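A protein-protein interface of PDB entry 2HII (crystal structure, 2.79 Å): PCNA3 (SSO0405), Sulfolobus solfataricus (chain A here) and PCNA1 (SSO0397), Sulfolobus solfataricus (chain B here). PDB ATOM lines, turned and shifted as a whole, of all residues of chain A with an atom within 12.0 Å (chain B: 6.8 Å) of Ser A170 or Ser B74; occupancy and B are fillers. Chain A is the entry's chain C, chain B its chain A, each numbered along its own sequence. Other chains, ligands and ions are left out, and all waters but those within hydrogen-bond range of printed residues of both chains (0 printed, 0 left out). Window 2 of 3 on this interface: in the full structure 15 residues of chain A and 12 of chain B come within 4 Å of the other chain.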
ATOM      1  N   SER A 141      28.595 -27.597  10.626  1.00  0.00           N
ATOM      2  CA  SER A 141      28.006 -26.615  11.530  1.00  0.00           C
ATOM      3  C   SER A 141      26.540 -26.935  11.803  1.00  0.00           C
ATOM      4  O   SER A 141      26.108 -26.936  12.953  1.00  0.00           O
ATOM      5  CB  SER A 141      28.122 -25.211  10.942  1.00  0.00           C
ATOM      6  OG  SER A 141      29.470 -24.848  10.738  1.00  0.00           O
ATOM      7  N   ALA A 142      25.794 -27.228  10.739  1.00  0.00           N
ATOM      8  CA  ALA A 142      24.365 -27.469  10.825  1.00  0.00           C
ATOM      9  C   ALA A 142      24.076 -28.612  11.772  1.00  0.00           C
ATOM     10  O   ALA A 142      23.378 -28.443  12.770  1.00  0.00           O
ATOM     11  CB  ALA A 142      23.806 -27.778   9.471  1.00  0.00           C
ATOM     12  N   ILE A 143      24.638 -29.775  11.470  1.00  0.00           N
ATOM     13  CA  ILE A 143      24.437 -30.951  12.314  1.00  0.00           C
ATOM     14  C   ILE A 143      24.986 -30.775  13.720  1.00  0.00           C
ATOM     15  O   ILE A 143      24.317 -31.135  14.683  1.00  0.00           O
ATOM     16  CB  ILE A 143      24.992 -32.213  11.665  1.00  0.00           C
ATOM     17  CG1 ILE A 143      23.934 -32.757  10.719  1.00  0.00           C
ATOM     18  CG2 ILE A 143      25.336 -33.255  12.699  1.00  0.00           C
ATOM     19  CD1 ILE A 143      24.334 -34.003  10.066  1.00  0.00           C
ATOM     20  N   SER A 144      26.183 -30.216  13.842  1.00  0.00           N
ATOM     21  CA  SER A 144      26.754 -29.948  15.153  1.00  0.00           C
ATOM     22  C   SER A 144      25.802 -29.133  16.019  1.00  0.00           C
ATOM     23  O   SER A 144      25.495 -29.535  17.141  1.00  0.00           O
ATOM     24  CB  SER A 144      28.099 -29.250  15.015  1.00  0.00           C
ATOM     25  OG  SER A 144      28.958 -30.006  14.181  1.00  0.00           O
ATOM     26  N   GLU A 145      25.310 -28.022  15.469  1.00  0.00           N
ATOM     27  CA  GLU A 145      24.355 -27.132  16.142  1.00  0.00           C
ATOM     28  C   GLU A 145      23.115 -27.837  16.678  1.00  0.00           C
ATOM     29  O   GLU A 145      22.717 -27.640  17.824  1.00  0.00           O
ATOM     30  CB  GLU A 145      23.907 -26.031  15.182  1.00  0.00           C
ATOM     31  CG  GLU A 145      24.884 -24.900  15.041  1.00  0.00           C
ATOM     32  CD  GLU A 145      24.560 -24.033  13.852  1.00  0.00           C
ATOM     33  OE1 GLU A 145      23.478 -23.415  13.848  1.00  0.00           O
ATOM     34  OE2 GLU A 145      25.389 -23.972  12.916  1.00  0.00           O
ATOM     35  N   VAL A 146      22.513 -28.651  15.822  1.00  0.00           N
ATOM     36  CA  VAL A 146      21.229 -29.283  16.080  1.00  0.00           C
ATOM     37  C   VAL A 146      21.383 -30.431  17.070  1.00  0.00           C
ATOM     38  O   VAL A 146      20.584 -30.582  17.989  1.00  0.00           O
ATOM     39  CB  VAL A 146      20.611 -29.778  14.752  1.00  0.00           C
ATOM     40  CG1 VAL A 146      19.319 -30.529  14.990  1.00  0.00           C
ATOM     41  CG2 VAL A 146      20.357 -28.603  13.821  1.00  0.00           C
ATOM     42  N   SER A 147      22.432 -31.223  16.885  1.00  0.00           N
ATOM     43  CA  SER A 147      22.701 -32.378  17.734  1.00  0.00           C
ATOM     44  C   SER A 147      22.852 -32.024  19.200  1.00  0.00           C
ATOM     45  O   SER A 147      22.585 -32.840  20.075  1.00  0.00           O
ATOM     46  CB  SER A 147      23.960 -33.098  17.263  1.00  0.00           C
ATOM     47  OG  SER A 147      23.713 -33.735  16.033  1.00  0.00           O
ATOM     48  N   THR A 148      23.287 -30.800  19.457  1.00  0.00           N
ATOM     49  CA  THR A 148      23.514 -30.328  20.811  1.00  0.00           C
ATOM     50  C   THR A 148      22.240 -30.378  21.669  1.00  0.00           C
ATOM     51  O   THR A 148      22.323 -30.467  22.891  1.00  0.00           O
ATOM     52  CB  THR A 148      24.172 -28.936  20.777  1.00  0.00           C
ATOM     53  OG1 THR A 148      25.510 -29.072  20.287  1.00  0.00           O
ATOM     54  CG2 THR A 148      24.259 -28.332  22.137  1.00  0.00           C
ATOM     55  N   VAL A 149      21.074 -30.380  21.029  1.00  0.00           N
ATOM     56  CA  VAL A 149      19.798 -30.366  21.753  1.00  0.00           C
ATOM     57  C   VAL A 149      18.872 -31.546  21.464  1.00  0.00           C
ATOM     58  O   VAL A 149      17.834 -31.687  22.105  1.00  0.00           O
ATOM     59  CB  VAL A 149      19.004 -29.041  21.521  1.00  0.00           C
ATOM     60  CG1 VAL A 149      19.720 -27.859  22.157  1.00  0.00           C
ATOM     61  CG2 VAL A 149      18.748 -28.791  20.031  1.00  0.00           C
ATOM     62  N   THR A 150      19.237 -32.372  20.492  1.00  0.00           N
ATOM     63  CA  THR A 150      18.411 -33.511  20.073  1.00  0.00           C
ATOM     64  C   THR A 150      19.267 -34.641  19.495  1.00  0.00           C
ATOM     65  O   THR A 150      20.356 -34.396  18.973  1.00  0.00           O
ATOM     66  CB  THR A 150      17.363 -33.088  19.011  1.00  0.00           C
ATOM     67  OG1 THR A 150      16.393 -34.126  18.841  1.00  0.00           O
ATOM     68  CG2 THR A 150      18.026 -32.794  17.666  1.00  0.00           C
ATOM     69  N   ASP A 151      18.775 -35.871  19.582  1.00  0.00           N
ATOM     70  CA  ASP A 151      19.431 -36.978  18.893  1.00  0.00           C
ATOM     71  C   ASP A 151      18.556 -37.518  17.763  1.00  0.00           C
ATOM     72  O   ASP A 151      18.713 -38.664  17.317  1.00  0.00           O
ATOM     73  CB  ASP A 151      19.873 -38.063  19.872  1.00  0.00           C
ATOM     74  CG  ASP A 151      18.800 -38.401  20.868  1.00  0.00           C
ATOM     75  OD1 ASP A 151      19.043 -38.253  22.094  1.00  0.00           O
ATOM     76  OD2 ASP A 151      17.700 -38.792  20.417  1.00  0.00           O
ATOM     77  N   ASN A 152      17.646 -36.656  17.309  1.00  0.00           N
ATOM     78  CA  ASN A 152      16.831 -36.853  16.110  1.00  0.00           C
ATOM     79  C   ASN A 152      16.903 -35.610  15.219  1.00  0.00           C
ATOM     80  O   ASN A 152      16.241 -34.595  15.502  1.00  0.00           O
ATOM     81  CB  ASN A 152      15.366 -37.093  16.476  1.00  0.00           C
ATOM     82  CG  ASN A 152      15.178 -38.267  17.405  1.00  0.00           C
ATOM     83  OD1 ASN A 152      15.763 -39.341  17.203  1.00  0.00           O
ATOM     84  ND2 ASN A 152      14.348 -38.074  18.436  1.00  0.00           N
ATOM     85  N   VAL A 153      17.705 -35.695  14.154  1.00  0.00           N
ATOM     86  CA  VAL A 153      17.930 -34.584  13.231  1.00  0.00           C
ATOM     87  C   VAL A 153      16.886 -34.613  12.126  1.00  0.00           C
ATOM     88  O   VAL A 153      16.828 -35.552  11.328  1.00  0.00           O
ATOM     89  CB  VAL A 153      19.345 -34.635  12.602  1.00  0.00           C
ATOM     90  CG1 VAL A 153      19.509 -33.565  11.535  1.00  0.00           C
ATOM     91  CG2 VAL A 153      20.407 -34.462  13.668  1.00  0.00           C
ATOM     92  N   VAL A 154      16.052 -33.583  12.087  1.00  0.00           N
ATOM     93  CA  VAL A 154      15.007 -33.532  11.088  1.00  0.00           C
ATOM     94  C   VAL A 154      15.572 -32.839   9.858  1.00  0.00           C
ATOM     95  O   VAL A 154      16.190 -31.785   9.955  1.00  0.00           O
ATOM     96  CB  VAL A 154      13.715 -32.851  11.619  1.00  0.00           C
ATOM     97  CG1 VAL A 154      12.645 -32.787  10.543  1.00  0.00           C
ATOM     98  CG2 VAL A 154      13.163 -33.620  12.811  1.00  0.00           C
ATOM     99  N   ILE A 164      17.844 -27.977   8.148  1.00  0.00           N
ATOM    100  CA  ILE A 164      18.261 -28.975   9.091  1.00  0.00           C
ATOM    101  C   ILE A 164      17.790 -28.446  10.423  1.00  0.00           C
ATOM    102  O   ILE A 164      18.115 -27.326  10.809  1.00  0.00           O
ATOM    103  CB  ILE A 164      19.764 -29.247   9.041  1.00  0.00           C
ATOM    104  CG1 ILE A 164      20.109 -29.975   7.732  1.00  0.00           C
ATOM    105  CG2 ILE A 164      20.166 -30.092  10.215  1.00  0.00           C
ATOM    106  CD1 ILE A 164      21.560 -30.446   7.606  1.00  0.00           C
ATOM    107  N   LYS A 165      16.973 -29.236  11.104  1.00  0.00           N
ATOM    108  CA  LYS A 165      16.272 -28.732  12.262  1.00  0.00           C
ATOM    109  C   LYS A 165      16.119 -29.727  13.390  1.00  0.00           C
ATOM    110  O   LYS A 165      16.226 -30.938  13.183  1.00  0.00           O
ATOM    111  CB  LYS A 165      14.915 -28.135  11.866  1.00  0.00           C
ATOM    112  CG  LYS A 165      13.945 -29.065  11.194  1.00  0.00           C
ATOM    113  CD  LYS A 165      13.173 -28.313  10.123  1.00  0.00           C
ATOM    114  CE  LYS A 165      12.129 -27.366  10.691  1.00  0.00           C
ATOM    115  NZ  LYS A 165      10.838 -28.075  10.912  1.00  0.00           N
ATOM    116  N   ALA A 166      15.903 -29.177  14.585  1.00  0.00           N
ATOM    117  CA  ALA A 166      15.517 -29.929  15.761  1.00  0.00           C
ATOM    118  C   ALA A 166      14.080 -29.553  16.099  1.00  0.00           C
ATOM    119  O   ALA A 166      13.657 -28.418  15.852  1.00  0.00           O
ATOM    120  CB  ALA A 166      16.435 -29.609  16.915  1.00  0.00           C
ATOM    121  N   GLU A 167      13.330 -30.504  16.656  1.00  0.00           N
ATOM    122  CA  GLU A 167      11.905 -30.279  16.926  1.00  0.00           C
ATOM    123  C   GLU A 167      11.426 -30.675  18.329  1.00  0.00           C
ATOM    124  O   GLU A 167      10.220 -30.613  18.600  1.00  0.00           O
ATOM    125  CB  GLU A 167      11.027 -30.909  15.829  1.00  0.00           C
ATOM    126  CG  GLU A 167      10.982 -30.082  14.516  1.00  0.00           C
ATOM    127  CD  GLU A 167      10.134 -30.713  13.398  1.00  0.00           C
ATOM    128  OE1 GLU A 167       9.225 -31.539  13.688  1.00  0.00           O
ATOM    129  OE2 GLU A 167      10.375 -30.363  12.219  1.00  0.00           O
ATOM    130  N   GLY A 168      12.365 -31.040  19.213  1.00  0.00           N
ATOM    131  CA  GLY A 168      12.072 -31.373  20.630  1.00  0.00           C
ATOM    132  C   GLY A 168      11.643 -30.214  21.529  1.00  0.00           C
ATOM    133  O   GLY A 168      10.911 -29.308  21.097  1.00  0.00           O
ATOM    134  N   GLU A 169      12.083 -30.237  22.788  1.00  0.00           N
ATOM    135  CA  GLU A 169      11.784 -29.130  23.716  1.00  0.00           C
ATOM    136  C   GLU A 169      12.533 -27.861  23.286  1.00  0.00           C
ATOM    137  O   GLU A 169      12.168 -26.748  23.676  1.00  0.00           O
ATOM    138  CB  GLU A 169      12.101 -29.492  25.189  1.00  0.00           C
ATOM    139  CG  GLU A 169      11.250 -28.709  26.253  1.00  0.00           C
ATOM    140  CD  GLU A 169      11.952 -28.496  27.620  1.00  0.00           C
ATOM    141  OE1 GLU A 169      11.251 -28.445  28.661  1.00  0.00           O
ATOM    142  OE2 GLU A 169      13.200 -28.366  27.663  1.00  0.00           O
ATOM    143  N   SER A 170      13.581 -28.045  22.486  1.00  0.00           N
ATOM    144  CA  SER A 170      14.300 -26.940  21.850  1.00  0.00           C
ATOM    145  C   SER A 170      13.901 -26.892  20.381  1.00  0.00           C
ATOM    146  O   SER A 170      13.668 -27.941  19.771  1.00  0.00           O
ATOM    147  CB  SER A 170      15.816 -27.164  21.933  1.00  0.00           C
ATOM    148  OG  SER A 170      16.214 -27.714  23.175  1.00  0.00           O
ATOM    149  N   GLU A 171      13.832 -25.692  19.807  1.00  0.00           N
ATOM    150  CA  GLU A 171      13.578 -25.563  18.369  1.00  0.00           C
ATOM    151  C   GLU A 171      14.698 -24.811  17.689  1.00  0.00           C
ATOM    152  O   GLU A 171      14.971 -23.655  17.999  1.00  0.00           O
ATOM    153  CB  GLU A 171      12.223 -24.912  18.084  1.00  0.00           C
ATOM    154  CG  GLU A 171      11.053 -25.890  18.031  1.00  0.00           C
ATOM    155  CD  GLU A 171       9.698 -25.231  18.312  1.00  0.00           C
ATOM    156  OE1 GLU A 171       9.540 -24.011  18.050  1.00  0.00           O
ATOM    157  OE2 GLU A 171       8.781 -25.942  18.798  1.00  0.00           O
ATOM    158  N   VAL A 172      15.356 -25.501  16.775  1.00  0.00           N
ATOM    159  CA  VAL A 172      16.475 -24.956  16.037  1.00  0.00           C
ATOM    160  C   VAL A 172      16.250 -25.301  14.591  1.00  0.00           C
ATOM    161  O   VAL A 172      15.837 -26.393  14.273  1.00  0.00           O
ATOM    162  CB  VAL A 172      17.804 -25.581  16.477  1.00  0.00           C
ATOM    163  CG1 VAL A 172      18.916 -25.112  15.593  1.00  0.00           C
ATOM    164  CG2 VAL A 172      18.113 -25.217  17.892  1.00  0.00           C
ATOM    165  N   GLU A 173      16.531 -24.366  13.709  1.00  0.00           N
ATOM    166  CA  GLU A 173      16.326 -24.591  12.302  1.00  0.00           C
ATOM    167  C   GLU A 173      17.458 -23.894  11.549  1.00  0.00           C
ATOM    168  O   GLU A 173      17.623 -22.673  11.644  1.00  0.00           O
ATOM    169  CB  GLU A 173      14.943 -24.076  11.922  1.00  0.00           C
ATOM    170  CG  GLU A 173      14.725 -23.812  10.464  1.00  0.00           C
ATOM    171  CD  GLU A 173      13.546 -22.898  10.237  1.00  0.00           C
ATOM    172  OE1 GLU A 173      12.477 -23.156  10.845  1.00  0.00           O
ATOM    173  OE2 GLU A 173      13.701 -21.924   9.457  1.00  0.00           O
ATOM    174  N   VAL A 174      18.264 -24.689  10.847  1.00  0.00           N
ATOM    175  CA  VAL A 174      19.399 -24.189  10.073  1.00  0.00           C
ATOM    176  C   VAL A 174      19.025 -24.254   8.603  1.00  0.00           C
ATOM    177  O   VAL A 174      18.870 -25.324   8.051  1.00  0.00           O
ATOM    178  CB  VAL A 174      20.675 -25.029  10.332  1.00  0.00           C
ATOM    179  CG1 VAL A 174      21.890 -24.361   9.748  1.00  0.00           C
ATOM    180  CG2 VAL A 174      20.879 -25.253  11.820  1.00  0.00           C
ATOM    181  N   LYS A 193      10.374 -34.532   4.358  1.00  0.00           N
ATOM    182  CA  LYS A 193      10.597 -34.266   5.764  1.00  0.00           C
ATOM    183  C   LYS A 193      10.801 -35.619   6.419  1.00  0.00           C
ATOM    184  O   LYS A 193       9.931 -36.492   6.318  1.00  0.00           O
ATOM    185  CB  LYS A 193       9.364 -33.595   6.363  1.00  0.00           C
ATOM    186  CG  LYS A 193       9.645 -32.639   7.499  1.00  0.00           C
ATOM    187  CD  LYS A 193       8.371 -32.387   8.304  1.00  0.00           C
ATOM    188  CE  LYS A 193       8.282 -30.942   8.818  1.00  0.00           C
ATOM    189  NZ  LYS A 193       9.388 -30.570   9.757  1.00  0.00           N
ATOM    190  N   ASP B  24      22.287 -20.719  34.377  1.00  0.00           N
ATOM    191  CA  ASP B  24      21.939 -20.561  32.963  1.00  0.00           C
ATOM    192  C   ASP B  24      20.750 -19.631  32.729  1.00  0.00           C
ATOM    193  O   ASP B  24      20.456 -19.261  31.584  1.00  0.00           O
ATOM    194  CB  ASP B  24      21.673 -21.918  32.318  1.00  0.00           C
ATOM    195  CG  ASP B  24      22.958 -22.648  31.953  1.00  0.00           C
ATOM    196  OD1 ASP B  24      23.728 -22.131  31.086  1.00  0.00           O
ATOM    197  OD2 ASP B  24      23.188 -23.742  32.541  1.00  0.00           O
ATOM    198  N   ASP B  71      16.011 -19.184  29.989  1.00  0.00           N
ATOM    199  CA  ASP B  71      17.070 -20.143  30.239  1.00  0.00           C
ATOM    200  C   ASP B  71      17.869 -20.253  28.977  1.00  0.00           C
ATOM    201  O   ASP B  71      17.336 -20.557  27.924  1.00  0.00           O
ATOM    202  CB  ASP B  71      16.506 -21.510  30.595  1.00  0.00           C
ATOM    203  CG  ASP B  71      17.600 -22.542  30.856  1.00  0.00           C
ATOM    204  OD1 ASP B  71      18.762 -22.326  30.441  1.00  0.00           O
ATOM    205  OD2 ASP B  71      17.294 -23.578  31.480  1.00  0.00           O
ATOM    206  N   VAL B  72      19.161 -20.027  29.078  1.00  0.00           N
ATOM    207  CA  VAL B  72      19.956 -19.864  27.881  1.00  0.00           C
ATOM    208  C   VAL B  72      20.961 -21.016  27.704  1.00  0.00           C
ATOM    209  O   VAL B  72      21.813 -20.985  26.819  1.00  0.00           O
ATOM    210  CB  VAL B  72      20.557 -18.443  27.847  1.00  0.00           C
ATOM    211  CG1 VAL B  72      21.907 -18.380  28.540  1.00  0.00           C
ATOM    212  CG2 VAL B  72      20.604 -17.933  26.439  1.00  0.00           C
ATOM    213  N   SER B  73      20.818 -22.045  28.537  1.00  0.00           N
ATOM    214  CA  SER B  73      21.684 -23.218  28.495  1.00  0.00           C
ATOM    215  C   SER B  73      21.811 -23.771  27.078  1.00  0.00           C
ATOM    216  O   SER B  73      22.913 -23.819  26.517  1.00  0.00           O
ATOM    217  CB  SER B  73      21.163 -24.310  29.434  1.00  0.00           C
ATOM    218  OG  SER B  73      19.768 -24.496  29.257  1.00  0.00           O
ATOM    219  N   SER B  74      20.681 -24.181  26.504  1.00  0.00           N
ATOM    220  CA  SER B  74      20.643 -24.690  25.133  1.00  0.00           C
ATOM    221  C   SER B  74      21.333 -23.765  24.129  1.00  0.00           C
ATOM    222  O   SER B  74      22.305 -24.155  23.475  1.00  0.00           O
ATOM    223  CB  SER B  74      19.206 -24.942  24.681  1.00  0.00           C
ATOM    224  OG  SER B  74      18.669 -26.084  25.312  1.00  0.00           O
ATOM    225  N   VAL B  75      20.824 -22.543  24.009  1.00  0.00           N
ATOM    226  CA  VAL B  75      21.362 -21.576  23.066  1.00  0.00           C
ATOM    227  C   VAL B  75      22.870 -21.535  23.208  1.00  0.00           C
ATOM    228  O   VAL B  75      23.584 -21.583  22.214  1.00  0.00           O
ATOM    229  CB  VAL B  75      20.793 -20.168  23.307  1.00  0.00           C
ATOM    230  CG1 VAL B  75      20.893 -19.339  22.044  1.00  0.00           C
ATOM    231  CG2 VAL B  75      19.353 -20.261  23.729  1.00  0.00           C
ATOM    232  N   LYS B  76      23.351 -21.470  24.449  1.00  0.00           N
ATOM    233  CA  LYS B  76      24.785 -21.407  24.693  1.00  0.00           C
ATOM    234  C   LYS B  76      25.487 -22.596  24.061  1.00  0.00           C
ATOM    235  O   LYS B  76      26.489 -22.431  23.360  1.00  0.00           O
ATOM    236  CB  LYS B  76      25.102 -21.294  26.187  1.00  0.00           C
ATOM    237  CG  LYS B  76      25.432 -19.864  26.637  1.00  0.00           C
ATOM    238  CD  LYS B  76      25.373 -19.728  28.150  1.00  0.00           C
ATOM    239  CE  LYS B  76      26.611 -20.239  28.837  1.00  0.00           C
ATOM    240  NZ  LYS B  76      26.336 -20.353  30.288  1.00  0.00           N
ATOM    241  N   LYS B  77      24.922 -23.781  24.284  1.00  0.00           N
ATOM    242  CA  LYS B  77      25.459 -25.036  23.752  1.00  0.00           C
ATOM    243  C   LYS B  77      25.599 -24.980  22.230  1.00  0.00           C
ATOM    244  O   LYS B  77      26.664 -25.288  21.690  1.00  0.00           O
ATOM    245  CB  LYS B  77      24.554 -26.217  24.126  1.00  0.00           C
ATOM    246  CG  LYS B  77      24.547 -26.646  25.585  1.00  0.00           C
ATOM    247  CD  LYS B  77      23.666 -27.901  25.731  1.00  0.00           C
ATOM    248  CE  LYS B  77      23.535 -28.370  27.181  1.00  0.00           C
ATOM    249  NZ  LYS B  77      22.599 -29.526  27.274  1.00  0.00           N
ATOM    250  N   ILE B  78      24.537 -24.572  21.539  1.00  0.00           N
ATOM    251  CA  ILE B  78      24.526 -24.710  20.083  1.00  0.00           C
ATOM    252  C   ILE B  78      25.357 -23.665  19.358  1.00  0.00           C
ATOM    253  O   ILE B  78      25.912 -23.942  18.300  1.00  0.00           O
ATOM    254  CB  ILE B  78      23.094 -24.869  19.447  1.00  0.00           C
ATOM    255  CG1 ILE B  78      22.385 -23.541  19.262  1.00  0.00           C
ATOM    256  CG2 ILE B  78      22.222 -25.808  20.267  1.00  0.00           C
ATOM    257  CD1 ILE B  78      20.897 -23.671  19.426  1.00  0.00           C
ATOM    258  N   LEU B  79      25.464 -22.474  19.932  1.00  0.00           N
ATOM    259  CA  LEU B  79      26.257 -21.415  19.302  1.00  0.00           C
ATOM    260  C   LEU B  79      27.764 -21.686  19.377  1.00  0.00           C
ATOM    261  O   LEU B  79      28.524 -21.243  18.495  1.00  0.00           O
ATOM    262  CB  LEU B  79      25.918 -20.056  19.893  1.00  0.00           C
ATOM    263  CG  LEU B  79      24.607 -19.517  19.335  1.00  0.00           C
ATOM    264  CD1 LEU B  79      24.035 -18.515  20.291  1.00  0.00           C
ATOM    265  CD2 LEU B  79      24.833 -18.888  17.977  1.00  0.00           C
ATOM    266  N   ILE B 113      17.142 -19.736  16.439  1.00  0.00           N
ATOM    267  CA  ILE B 113      16.919 -20.408  17.721  1.00  0.00           C
ATOM    268  C   ILE B 113      15.683 -19.870  18.429  1.00  0.00           C
ATOM    269  O   ILE B 113      15.586 -18.677  18.722  1.00  0.00           O
ATOM    270  CB  ILE B 113      18.129 -20.264  18.689  1.00  0.00           C
ATOM    271  CG1 ILE B 113      19.475 -20.379  17.956  1.00  0.00           C
ATOM    272  CG2 ILE B 113      18.006 -21.237  19.866  1.00  0.00           C
ATOM    273  CD1 ILE B 113      19.671 -21.648  17.125  1.00  0.00           C
ATOM    274  N   TYR B 114      14.748 -20.772  18.705  1.00  0.00           N
ATOM    275  CA  TYR B 114      13.496 -20.440  19.369  1.00  0.00           C
ATOM    276  C   TYR B 114      13.583 -20.751  20.846  1.00  0.00           C
ATOM    277  O   TYR B 114      13.619 -21.920  21.212  1.00  0.00           O
ATOM    278  CB  TYR B 114      12.359 -21.258  18.753  1.00  0.00           C
ATOM    279  CG  TYR B 114      11.921 -20.752  17.407  1.00  0.00           C
ATOM    280  CD1 TYR B 114      12.348 -21.360  16.236  1.00  0.00           C
ATOM    281  CD2 TYR B 114      11.088 -19.652  17.305  1.00  0.00           C
ATOM    282  CE1 TYR B 114      11.953 -20.879  14.991  1.00  0.00           C
ATOM    283  CE2 TYR B 114      10.691 -19.167  16.075  1.00  0.00           C
ATOM    284  CZ  TYR B 114      11.123 -19.782  14.923  1.00  0.00           C
ATOM    285  OH  TYR B 114      10.717 -19.281  13.710  1.00  0.00           O
ATOM    286  N   ILE B 115      13.629 -19.721  21.694  1.00  0.00           N
ATOM    287  CA  ILE B 115      13.534 -19.960  23.139  1.00  0.00           C
ATOM    288  C   ILE B 115      12.364 -19.274  23.858  1.00  0.00           C
ATOM    289  O   ILE B 115      11.983 -18.138  23.547  1.00  0.00           O
ATOM    290  CB  ILE B 115      14.862 -19.771  23.887  1.00  0.00           C
ATOM    291  CG1 ILE B 115      15.517 -18.452  23.540  1.00  0.00           C
ATOM    292  CG2 ILE B 115      15.808 -20.937  23.580  1.00  0.00           C
ATOM    293  CD1 ILE B 115      16.502 -18.075  24.564  1.00  0.00           C
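N of Ala A166 sits at hydrogen-bond distance from O of Val A172 (2.8 Å). O of Ser A144 lies within hydrogen-bond range of OG1 of Thr A148 (3.2 Å).
Of the 26 printed residues of chain A, 6 touch a printed residue of chain B. Of the 13 printed residues of chain B, 5 touch a printed residue of chain A. Among the printed residues, 10 pairs touch across the chains.
Ile B78 touches Glu A145 (CG2 to O, 3.1 Å). Thr A148 touches Lys B77 (CG2 to CB, 2.9 Å). Ile B78 touches Thr A148. Val A149 touches Ser B74 (CG1 to OG, 3.8 Å). Ile B78 touches Val A149 (CG2 to CG1, 3.7 Å). OG of Ser B74 touches OG of Ser A170 (3.6 Å). O of Glu A171 touches CA of Ile B113, 3.8 Å away. Val A172 touches Ile B78 (CG2 to CD1, 3.5 Å). Val A172 touches Ile B113.
Ser A170 touches just one residue of chain B: Ser B74 (3.6 Å). Ser B74 touches just these residues of chain A: Val A149 (3.8 Å) and Ser A170 (3.6 Å). No residue of chain A comes within 4 Å of Asp B71. No residue of chain A comes within 4 Å of Val B72. Ser B73 touches none of the printed residues of chain A. Val B75 touches none of the printed residues of chain A. No residue of chain A comes within 4 Å of Lys B76. Of the printed residues of chain B, Glu A145 touches Ile B78 (3.1 Å). Printed residues of chain B within 4 Å of Glu A171: Ile B113 and Tyr B114. Printed residues of chain B within 4 Å of Thr A148: Lys B77 and Ile B78. Val A174 touches none of the printed residues of chain B. The nearest residue of chain A that does not touch Ser B74 is Thr A148 (4.8 Å).
The backbone NH (N) of Tyr B114 sits at hydrogen-bond distance from the backbone carbonyl oxygen (O) of Glu A171 (3.0 Å).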
